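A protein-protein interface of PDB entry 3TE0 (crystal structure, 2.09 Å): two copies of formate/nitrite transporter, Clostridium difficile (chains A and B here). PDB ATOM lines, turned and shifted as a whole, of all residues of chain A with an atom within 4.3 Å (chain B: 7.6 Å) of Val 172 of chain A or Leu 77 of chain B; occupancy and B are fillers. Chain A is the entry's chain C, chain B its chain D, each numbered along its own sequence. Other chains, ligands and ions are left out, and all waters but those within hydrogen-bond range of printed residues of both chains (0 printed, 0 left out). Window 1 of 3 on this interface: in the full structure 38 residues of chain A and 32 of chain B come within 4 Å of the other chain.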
ATOM      1  N   ILE A 168      -7.462  -8.138   1.176  1.00  0.00           N
ATOM      2  CA  ILE A 168      -8.320  -9.274   1.517  1.00  0.00           C
ATOM      3  C   ILE A 168      -9.226  -8.833   2.675  1.00  0.00           C
ATOM      4  O   ILE A 168     -10.444  -8.999   2.636  1.00  0.00           O
ATOM      5  CB  ILE A 168      -7.497 -10.532   1.882  1.00  0.00           C
ATOM      6  CG1 ILE A 168      -6.905 -11.148   0.607  1.00  0.00           C
ATOM      7  CG2 ILE A 168      -8.382 -11.581   2.594  1.00  0.00           C
ATOM      8  CD1 ILE A 168      -5.968 -12.350   0.832  1.00  0.00           C
ATOM      9  N   LEU A 169      -8.630  -8.204   3.681  1.00  0.00           N
ATOM     10  CA  LEU A 169      -9.398  -7.798   4.843  1.00  0.00           C
ATOM     11  C   LEU A 169     -10.376  -6.657   4.549  1.00  0.00           C
ATOM     12  O   LEU A 169     -11.529  -6.700   4.978  1.00  0.00           O
ATOM     13  CB  LEU A 169      -8.471  -7.444   6.008  1.00  0.00           C
ATOM     14  CG  LEU A 169      -8.103  -8.698   6.815  1.00  0.00           C
ATOM     15  CD1 LEU A 169      -6.839  -8.495   7.642  1.00  0.00           C
ATOM     16  CD2 LEU A 169      -9.295  -9.110   7.711  1.00  0.00           C
ATOM     17  N   VAL A 170      -9.918  -5.635   3.832  1.00  0.00           N
ATOM     18  CA  VAL A 170     -10.808  -4.533   3.484  1.00  0.00           C
ATOM     19  C   VAL A 170     -11.923  -5.027   2.563  1.00  0.00           C
ATOM     20  O   VAL A 170     -13.094  -4.694   2.758  1.00  0.00           O
ATOM     21  CB  VAL A 170     -10.038  -3.351   2.848  1.00  0.00           C
ATOM     22  CG1 VAL A 170     -10.991  -2.337   2.258  1.00  0.00           C
ATOM     23  CG2 VAL A 170      -9.113  -2.691   3.915  1.00  0.00           C
ATOM     24  N   CYS A 171     -11.584  -5.824   1.553  1.00  0.00           N
ATOM     25  CA  CYS A 171     -12.646  -6.244   0.641  1.00  0.00           C
ATOM     26  C   CYS A 171     -13.599  -7.247   1.288  1.00  0.00           C
ATOM     27  O   CYS A 171     -14.785  -7.235   0.978  1.00  0.00           O
ATOM     28  CB  CYS A 171     -12.099  -6.771  -0.692  1.00  0.00           C
ATOM     29  SG  CYS A 171     -11.497  -5.450  -1.737  1.00  0.00           S
ATOM     30  N   VAL A 172     -13.094  -8.105   2.180  1.00  0.00           N
ATOM     31  CA  VAL A 172     -13.990  -9.047   2.848  1.00  0.00           C
ATOM     32  C   VAL A 172     -14.972  -8.293   3.738  1.00  0.00           C
ATOM     33  O   VAL A 172     -16.131  -8.681   3.872  1.00  0.00           O
ATOM     34  CB  VAL A 172     -13.266 -10.192   3.620  1.00  0.00           C
ATOM     35  CG1 VAL A 172     -12.773  -9.716   5.010  1.00  0.00           C
ATOM     36  CG2 VAL A 172     -14.228 -11.369   3.783  1.00  0.00           C
ATOM     37  N   SER A 173     -14.524  -7.182   4.314  1.00  0.00           N
ATOM     38  CA  SER A 173     -15.428  -6.378   5.111  1.00  0.00           C
ATOM     39  C   SER A 173     -16.477  -5.720   4.197  1.00  0.00           C
ATOM     40  O   SER A 173     -17.655  -5.629   4.556  1.00  0.00           O
ATOM     41  CB  SER A 173     -14.658  -5.360   5.978  1.00  0.00           C
ATOM     42  OG  SER A 173     -14.456  -4.149   5.283  1.00  0.00           O
ATOM     43  N   VAL A 174     -16.071  -5.309   2.997  1.00  0.00           N
ATOM     44  CA  VAL A 174     -17.043  -4.793   2.023  1.00  0.00           C
ATOM     45  C   VAL A 174     -17.988  -5.915   1.597  1.00  0.00           C
ATOM     46  O   VAL A 174     -19.190  -5.697   1.395  1.00  0.00           O
ATOM     47  CB  VAL A 174     -16.369  -4.235   0.738  1.00  0.00           C
ATOM     48  CG1 VAL A 174     -17.434  -3.852  -0.305  1.00  0.00           C
ATOM     49  CG2 VAL A 174     -15.473  -3.036   1.059  1.00  0.00           C
ATOM     50  N   LEU A 175     -17.431  -7.116   1.438  1.00  0.00           N
ATOM     51  CA  LEU A 175     -18.225  -8.295   1.076  1.00  0.00           C
ATOM     52  C   LEU A 175     -19.294  -8.602   2.139  1.00  0.00           C
ATOM     53  O   LEU A 175     -20.442  -8.891   1.811  1.00  0.00           O
ATOM     54  CB  LEU A 175     -17.317  -9.522   0.889  1.00  0.00           C
ATOM     55  CG  LEU A 175     -18.047 -10.815   0.472  1.00  0.00           C
ATOM     56  CD1 LEU A 175     -18.803 -10.642  -0.879  1.00  0.00           C
ATOM     57  CD2 LEU A 175     -17.054 -11.955   0.401  1.00  0.00           C
ATOM     58  N   CYS A 176     -18.916  -8.552   3.415  1.00  0.00           N
ATOM     59  CA  CYS A 176     -19.903  -8.742   4.483  1.00  0.00           C
ATOM     60  C   CYS A 176     -21.031  -7.712   4.380  1.00  0.00           C
ATOM     61  O   CYS A 176     -22.196  -8.017   4.643  1.00  0.00           O
ATOM     62  CB  CYS A 176     -19.234  -8.672   5.868  1.00  0.00           C
ATOM     63  SG  CYS A 176     -18.122 -10.079   6.177  1.00  0.00           S
ATOM     64  N   MET A 189     -18.331  -5.756  11.510  1.00  0.00           N
ATOM     65  CA  MET A 189     -17.405  -6.565  10.703  1.00  0.00           C
ATOM     66  C   MET A 189     -16.254  -5.688  10.223  1.00  0.00           C
ATOM     67  O   MET A 189     -15.108  -6.128  10.153  1.00  0.00           O
ATOM     68  CB  MET A 189     -18.103  -7.256   9.517  1.00  0.00           C
ATOM     69  CG  MET A 189     -19.090  -8.365   9.935  1.00  0.00           C
ATOM     70  SD  MET A 189     -18.360  -9.545  11.121  1.00  0.00           S
ATOM     71  CE  MET A 189     -17.016 -10.252  10.160  1.00  0.00           C
ATOM     72  N   CYS A 193     -12.255  -6.327  10.916  1.00  0.00           N
ATOM     73  CA  CYS A 193     -11.310  -6.465   9.808  1.00  0.00           C
ATOM     74  C   CYS A 193     -10.204  -5.408   9.858  1.00  0.00           C
ATOM     75  O   CYS A 193      -9.047  -5.703   9.561  1.00  0.00           O
ATOM     76  CB  CYS A 193     -12.033  -6.422   8.457  1.00  0.00           C
ATOM     77  SG  CYS A 193     -13.110  -7.870   8.156  1.00  0.00           S
ATOM     78  N   MET A 248     -10.280 -11.931  -3.641  1.00  0.00           N
ATOM     79  CA  MET A 248     -11.692 -11.681  -3.315  1.00  0.00           C
ATOM     80  C   MET A 248     -12.635 -11.629  -4.529  1.00  0.00           C
ATOM     81  O   MET A 248     -13.732 -12.180  -4.479  1.00  0.00           O
ATOM     82  CB  MET A 248     -11.850 -10.433  -2.429  1.00  0.00           C
ATOM     83  CG  MET A 248     -11.091 -10.535  -1.073  1.00  0.00           C
ATOM     84  SD  MET A 248     -11.533 -11.973  -0.068  1.00  0.00           S
ATOM     85  CE  MET A 248     -13.318 -11.805  -0.057  1.00  0.00           C
ATOM     86  N   PHE B  36     -11.254 -20.389   1.519  1.00  0.00           N
ATOM     87  CA  PHE B  36     -11.612 -19.115   2.133  1.00  0.00           C
ATOM     88  C   PHE B  36     -11.758 -19.240   3.665  1.00  0.00           C
ATOM     89  O   PHE B  36     -11.176 -18.461   4.433  1.00  0.00           O
ATOM     90  CB  PHE B  36     -12.933 -18.555   1.560  1.00  0.00           C
ATOM     91  CG  PHE B  36     -12.756 -17.625   0.397  1.00  0.00           C
ATOM     92  CD1 PHE B  36     -11.963 -16.487   0.506  1.00  0.00           C
ATOM     93  CD2 PHE B  36     -13.419 -17.867  -0.814  1.00  0.00           C
ATOM     94  CE1 PHE B  36     -11.815 -15.608  -0.564  1.00  0.00           C
ATOM     95  CE2 PHE B  36     -13.277 -16.991  -1.898  1.00  0.00           C
ATOM     96  CZ  PHE B  36     -12.470 -15.864  -1.774  1.00  0.00           C
ATOM     97  N   ALA B  37     -12.569 -20.192   4.109  1.00  0.00           N
ATOM     98  CA  ALA B  37     -12.806 -20.336   5.550  1.00  0.00           C
ATOM     99  C   ALA B  37     -11.505 -20.625   6.335  1.00  0.00           C
ATOM    100  O   ALA B  37     -11.273 -20.051   7.399  1.00  0.00           O
ATOM    101  CB  ALA B  37     -13.866 -21.409   5.829  1.00  0.00           C
ATOM    102  N   LEU B  39      -8.576 -19.706   5.465  1.00  0.00           N
ATOM    103  CA  LEU B  39      -7.848 -18.447   5.462  1.00  0.00           C
ATOM    104  C   LEU B  39      -8.438 -17.407   6.442  1.00  0.00           C
ATOM    105  O   LEU B  39      -7.694 -16.670   7.102  1.00  0.00           O
ATOM    106  CB  LEU B  39      -7.771 -17.883   4.043  1.00  0.00           C
ATOM    107  CG  LEU B  39      -6.952 -16.607   3.833  1.00  0.00           C
ATOM    108  CD1 LEU B  39      -6.203 -16.663   2.477  1.00  0.00           C
ATOM    109  CD2 LEU B  39      -7.851 -15.380   3.932  1.00  0.00           C
ATOM    110  N   TYR B  40      -9.766 -17.349   6.527  1.00  0.00           N
ATOM    111  CA  TYR B  40     -10.445 -16.420   7.420  1.00  0.00           C
ATOM    112  C   TYR B  40     -10.118 -16.776   8.857  1.00  0.00           C
ATOM    113  O   TYR B  40      -9.844 -15.898   9.681  1.00  0.00           O
ATOM    114  CB  TYR B  40     -11.967 -16.449   7.208  1.00  0.00           C
ATOM    115  CG  TYR B  40     -12.424 -15.889   5.880  1.00  0.00           C
ATOM    116  CD1 TYR B  40     -11.672 -14.931   5.214  1.00  0.00           C
ATOM    117  CD2 TYR B  40     -13.614 -16.328   5.285  1.00  0.00           C
ATOM    118  CE1 TYR B  40     -12.095 -14.398   3.987  1.00  0.00           C
ATOM    119  CE2 TYR B  40     -14.038 -15.807   4.055  1.00  0.00           C
ATOM    120  CZ  TYR B  40     -13.268 -14.856   3.413  1.00  0.00           C
ATOM    121  OH  TYR B  40     -13.683 -14.340   2.207  1.00  0.00           O
ATOM    122  N   VAL B  41     -10.130 -18.069   9.154  1.00  0.00           N
ATOM    123  CA  VAL B  41      -9.745 -18.511  10.496  1.00  0.00           C
ATOM    124  C   VAL B  41      -8.286 -18.128  10.737  1.00  0.00           C
ATOM    125  O   VAL B  41      -7.932 -17.605  11.797  1.00  0.00           O
ATOM    126  CB  VAL B  41      -9.978 -20.026  10.706  1.00  0.00           C
ATOM    127  CG1 VAL B  41      -9.382 -20.499  12.040  1.00  0.00           C
ATOM    128  CG2 VAL B  41     -11.490 -20.353  10.686  1.00  0.00           C
ATOM    129  N   ILE B  43      -6.589 -15.799   9.615  1.00  0.00           N
ATOM    130  CA  ILE B  43      -6.417 -14.365   9.777  1.00  0.00           C
ATOM    131  C   ILE B  43      -6.597 -13.997  11.248  1.00  0.00           C
ATOM    132  O   ILE B  43      -5.934 -13.078  11.761  1.00  0.00           O
ATOM    133  CB  ILE B  43      -7.417 -13.580   8.879  1.00  0.00           C
ATOM    134  CG1 ILE B  43      -6.850 -13.432   7.460  1.00  0.00           C
ATOM    135  CG2 ILE B  43      -7.755 -12.202   9.481  1.00  0.00           C
ATOM    136  CD1 ILE B  43      -7.789 -12.706   6.529  1.00  0.00           C
ATOM    137  N   GLY B  44      -7.493 -14.709  11.928  1.00  0.00           N
ATOM    138  CA  GLY B  44      -7.689 -14.482  13.350  1.00  0.00           C
ATOM    139  C   GLY B  44      -6.399 -14.863  14.077  1.00  0.00           C
ATOM    140  O   GLY B  44      -5.967 -14.193  15.024  1.00  0.00           O
ATOM    141  N   PHE B  71     -10.097 -12.683  18.977  1.00  0.00           N
ATOM    142  CA  PHE B  71     -10.141 -13.767  17.998  1.00  0.00           C
ATOM    143  C   PHE B  71     -11.476 -13.837  17.237  1.00  0.00           C
ATOM    144  O   PHE B  71     -11.581 -14.575  16.254  1.00  0.00           O
ATOM    145  CB  PHE B  71      -9.812 -15.114  18.689  1.00  0.00           C
ATOM    146  CG  PHE B  71      -9.596 -16.261  17.726  1.00  0.00           C
ATOM    147  CD1 PHE B  71      -8.532 -16.232  16.809  1.00  0.00           C
ATOM    148  CD2 PHE B  71     -10.441 -17.371  17.743  1.00  0.00           C
ATOM    149  CE1 PHE B  71      -8.325 -17.288  15.923  1.00  0.00           C
ATOM    150  CE2 PHE B  71     -10.243 -18.429  16.851  1.00  0.00           C
ATOM    151  CZ  PHE B  71      -9.172 -18.387  15.945  1.00  0.00           C
ATOM    152  N   ALA B  72     -12.483 -13.071  17.681  1.00  0.00           N
ATOM    153  CA  ALA B  72     -13.856 -13.142  17.111  1.00  0.00           C
ATOM    154  C   ALA B  72     -13.916 -13.114  15.566  1.00  0.00           C
ATOM    155  O   ALA B  72     -14.762 -13.757  14.948  1.00  0.00           O
ATOM    156  CB  ALA B  72     -14.725 -12.022  17.654  1.00  0.00           C
ATOM    157  N   ILE B  73     -13.024 -12.350  14.958  1.00  0.00           N
ATOM    158  CA  ILE B  73     -12.993 -12.236  13.500  1.00  0.00           C
ATOM    159  C   ILE B  73     -12.944 -13.601  12.808  1.00  0.00           C
ATOM    160  O   ILE B  73     -13.535 -13.760  11.748  1.00  0.00           O
ATOM    161  CB  ILE B  73     -11.827 -11.344  13.026  1.00  0.00           C
ATOM    162  CG1 ILE B  73     -11.965 -11.032  11.529  1.00  0.00           C
ATOM    163  CG2 ILE B  73     -10.458 -11.988  13.393  1.00  0.00           C
ATOM    164  CD1 ILE B  73     -10.912 -10.052  10.993  1.00  0.00           C
ATOM    165  N   ALA B  74     -12.251 -14.582  13.401  1.00  0.00           N
ATOM    166  CA  ALA B  74     -12.082 -15.887  12.752  1.00  0.00           C
ATOM    167  C   ALA B  74     -13.409 -16.538  12.326  1.00  0.00           C
ATOM    168  O   ALA B  74     -13.628 -16.803  11.149  1.00  0.00           O
ATOM    169  CB  ALA B  74     -11.249 -16.866  13.631  1.00  0.00           C
ATOM    170  N   LEU B  75     -14.294 -16.791  13.277  1.00  0.00           N
ATOM    171  CA  LEU B  75     -15.566 -17.421  12.949  1.00  0.00           C
ATOM    172  C   LEU B  75     -16.607 -16.408  12.435  1.00  0.00           C
ATOM    173  O   LEU B  75     -17.537 -16.777  11.704  1.00  0.00           O
ATOM    174  CB  LEU B  75     -16.099 -18.212  14.157  1.00  0.00           C
ATOM    175  CG  LEU B  75     -17.212 -19.243  13.936  1.00  0.00           C
ATOM    176  CD1 LEU B  75     -16.909 -20.232  12.793  1.00  0.00           C
ATOM    177  CD2 LEU B  75     -17.474 -19.996  15.227  1.00  0.00           C
ATOM    178  N   SER B  76     -16.463 -15.142  12.817  1.00  0.00           N
ATOM    179  CA  SER B  76     -17.376 -14.109  12.315  1.00  0.00           C
ATOM    180  C   SER B  76     -17.300 -14.017  10.782  1.00  0.00           C
ATOM    181  O   SER B  76     -18.331 -13.930  10.104  1.00  0.00           O
ATOM    182  CB  SER B  76     -17.112 -12.741  12.970  1.00  0.00           C
ATOM    183  OG  SER B  76     -17.245 -12.821  14.390  1.00  0.00           O
ATOM    184  N   LEU B  77     -16.087 -14.049  10.241  1.00  0.00           N
ATOM    185  CA  LEU B  77     -15.904 -14.011   8.786  1.00  0.00           C
ATOM    186  C   LEU B  77     -16.529 -15.244   8.118  1.00  0.00           C
ATOM    187  O   LEU B  77     -17.204 -15.144   7.083  1.00  0.00           O
ATOM    188  CB  LEU B  77     -14.415 -13.935   8.434  1.00  0.00           C
ATOM    189  CG  LEU B  77     -13.753 -12.560   8.603  1.00  0.00           C
ATOM    190  CD1 LEU B  77     -12.282 -12.630   8.226  1.00  0.00           C
ATOM    191  CD2 LEU B  77     -14.465 -11.490   7.743  1.00  0.00           C
ATOM    192  N   VAL B  78     -16.284 -16.408   8.702  1.00  0.00           N
ATOM    193  CA  VAL B  78     -16.806 -17.658   8.151  1.00  0.00           C
ATOM    194  C   VAL B  78     -18.331 -17.601   8.077  1.00  0.00           C
ATOM    195  O   VAL B  78     -18.921 -17.871   7.029  1.00  0.00           O
ATOM    196  CB  VAL B  78     -16.343 -18.854   9.003  1.00  0.00           C
ATOM    197  CG1 VAL B  78     -17.111 -20.131   8.641  1.00  0.00           C
ATOM    198  CG2 VAL B  78     -14.839 -19.046   8.857  1.00  0.00           C
ATOM    199  N   ILE B  79     -18.962 -17.221   9.186  1.00  0.00           N
ATOM    200  CA  ILE B  79     -20.414 -17.147   9.229  1.00  0.00           C
ATOM    201  C   ILE B  79     -20.975 -16.069   8.295  1.00  0.00           C
ATOM    202  O   ILE B  79     -21.961 -16.309   7.604  1.00  0.00           O
ATOM    203  CB  ILE B  79     -20.933 -16.930  10.672  1.00  0.00           C
ATOM    204  CG1 ILE B  79     -20.536 -18.120  11.556  1.00  0.00           C
ATOM    205  CG2 ILE B  79     -22.448 -16.737  10.686  1.00  0.00           C
ATOM    206  CD1 ILE B  79     -20.980 -19.430  11.016  1.00  0.00           C
ATOM    207  N   MET B  80     -20.345 -14.892   8.263  1.00  0.00           N
ATOM    208  CA  MET B  80     -20.877 -13.773   7.483  1.00  0.00           C
ATOM    209  C   MET B  80     -20.619 -13.916   5.979  1.00  0.00           C
ATOM    210  O   MET B  80     -21.295 -13.267   5.167  1.00  0.00           O
ATOM    211  CB  MET B  80     -20.358 -12.421   8.011  1.00  0.00           C
ATOM    212  CG  MET B  80     -20.815 -12.125   9.444  1.00  0.00           C
ATOM    213  SD  MET B  80     -22.606 -11.894   9.545  1.00  0.00           S
ATOM    214  CE  MET B  80     -22.720 -10.242   8.852  1.00  0.00           C
ATOM    215  N   THR B  81     -19.663 -14.772   5.611  1.00  0.00           N
ATOM    216  CA  THR B  81     -19.355 -15.050   4.195  1.00  0.00           C
ATOM    217  C   THR B  81     -19.996 -16.345   3.682  1.00  0.00           C
ATOM    218  O   THR B  81     -19.928 -16.638   2.486  1.00  0.00           O
ATOM    219  CB  THR B  81     -17.817 -15.137   3.912  1.00  0.00           C
ATOM    220  OG1 THR B  81     -17.224 -16.177   4.718  1.00  0.00           O
ATOM    221  CG2 THR B  81     -17.134 -13.783   4.220  1.00  0.00           C
ATOM    222  N   GLY B  82     -20.590 -17.130   4.583  1.00  0.00           N
ATOM    223  CA  GLY B  82     -21.180 -18.410   4.213  1.00  0.00           C
ATOM    224  C   GLY B  82     -20.214 -19.458   3.680  1.00  0.00           C
ATOM    225  O   GLY B  82     -20.575 -20.270   2.813  1.00  0.00           O
ATOM    226  N   THR B  83     -18.986 -19.465   4.199  1.00  0.00           N
ATOM    227  CA  THR B  83     -17.966 -20.398   3.707  1.00  0.00           C
ATOM    228  C   THR B  83     -17.854 -21.668   4.559  1.00  0.00           C
ATOM    229  O   THR B  83     -18.401 -21.741   5.656  1.00  0.00           O
ATOM    230  CB  THR B  83     -16.610 -19.702   3.565  1.00  0.00           C
ATOM    231  OG1 THR B  83     -16.376 -18.904   4.731  1.00  0.00           O
ATOM    232  CG2 THR B  83     -16.627 -18.786   2.338  1.00  0.00           C
ATOM    233  N   ILE B 187     -22.830 -12.493  15.713  1.00  0.00           N
ATOM    234  CA  ILE B 187     -21.434 -12.089  15.881  1.00  0.00           C
ATOM    235  C   ILE B 187     -21.103 -11.973  17.358  1.00  0.00           C
ATOM    236  O   ILE B 187     -20.033 -12.382  17.799  1.00  0.00           O
ATOM    237  CB  ILE B 187     -21.150 -10.741  15.175  1.00  0.00           C
ATOM    238  CG1 ILE B 187     -21.253 -10.916  13.651  1.00  0.00           C
ATOM    239  CG2 ILE B 187     -19.784 -10.187  15.584  1.00  0.00           C
ATOM    240  CD1 ILE B 187     -21.556  -9.601  12.917  1.00  0.00           C
ATOM    241  N   ILE B 190     -20.582 -15.500  18.704  1.00  0.00           N
ATOM    242  CA  ILE B 190     -19.278 -15.924  18.222  1.00  0.00           C
ATOM    243  C   ILE B 190     -18.135 -15.273  19.029  1.00  0.00           C
ATOM    244  O   ILE B 190     -17.183 -15.940  19.449  1.00  0.00           O
ATOM    245  CB  ILE B 190     -19.110 -15.578  16.740  1.00  0.00           C
ATOM    246  CG1 ILE B 190     -20.002 -16.499  15.895  1.00  0.00           C
ATOM    247  CG2 ILE B 190     -17.612 -15.651  16.339  1.00  0.00           C
ATOM    248  CD1 ILE B 190     -20.250 -16.015  14.451  1.00  0.00           C
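Among the printed residues, pairs that only touch across the chains: Leu 169 of chain A with Ile 43 of chain B (3.9 Å), Leu 169 of chain A with Ile 73 of chain B (3.8 Å), Val 172 of chain A with Tyr 40 of chain B (3.4 Å), Val 172 of chain A with Leu 77 of chain B (3.7 Å), Val 172 of chain A with Thr 81 of chain B (3.8 Å), Cys 176 of chain A with Met 80 of chain B (3.7 Å), Met 189 of chain A with Ser 76 of chain B (3.8 Å), Met 189 of chain A with Leu 77 of chain B (3.7 Å), Met 189 of chain A with Met 80 of chain B (3.9 Å), Met 189 of chain A with Ile 187 of chain B (3.7 Å), Cys 193 of chain A with Ile 73 of chain B (3.8 Å), Cys 193 of chain A with Leu 77 of chain B (3.9 Å), Met 248 of chain A with Phe 36 of chain B (3.7 Å) and Met 248 of chain A with Tyr 40 of chain B (3.4 Å).
The backbone carbonyl oxygen (O) of Leu 169 of chain A lies close to the side-chain sulfur (SG) of Cys 193 of chain A (3.7 Å). The backbone carbonyl oxygen of Val 172 of chain A sits at hydrogen-bond distance from the side-chain sulfur of Cys 176 of chain A (3.4 Å). The backbone carbonyl oxygen (O) of Met 189 of chain A sits at hydrogen-bond distance from the side-chain sulfur (SG) of Cys 193 of chain A (3.3 Å). O of Ala 72 of chain B sits at hydrogen-bond distance from OG of Ser 76 of chain B. OG1 of Thr 81 of chain B lies within hydrogen-bond range of O of Leu 77 of chain B, 2.6 Å away. OG1 of Thr 81 of chain B lies within hydrogen-bond range of OG1 of Thr 83 of chain B, 2.9 Å away.
Leu 77 of chain B touches just these residues of chain A: Val 172, Met 189 and Cys 193. Of the printed residues of chain B, Cys 193 of chain A touches Ile 73 (3.8 Å) and Leu 77 (3.9 Å). Of the printed residues of chain B, Met 248 of chain A touches Phe 36 (3.7 Å) and Tyr 40 (3.4 Å). Of the printed residues of chain A, Tyr 40 of chain B touches Val 172 and Met 248. The nearest residue of chain A that does not touch Leu 77 of chain B is Cys 176 of chain A (4.2 Å). The nearest printed residue of chain B that does not touch Leu 169 of chain A is Leu 77 of chain B (4.6 Å).
No position is printed for both chains.
Among the printed residues, 14 pairs touch across the chains. Among the printed residues, no Asp or Glu carboxylate lies within 4 Å of a Lys or Arg side-chain nitrogen of the other chain.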
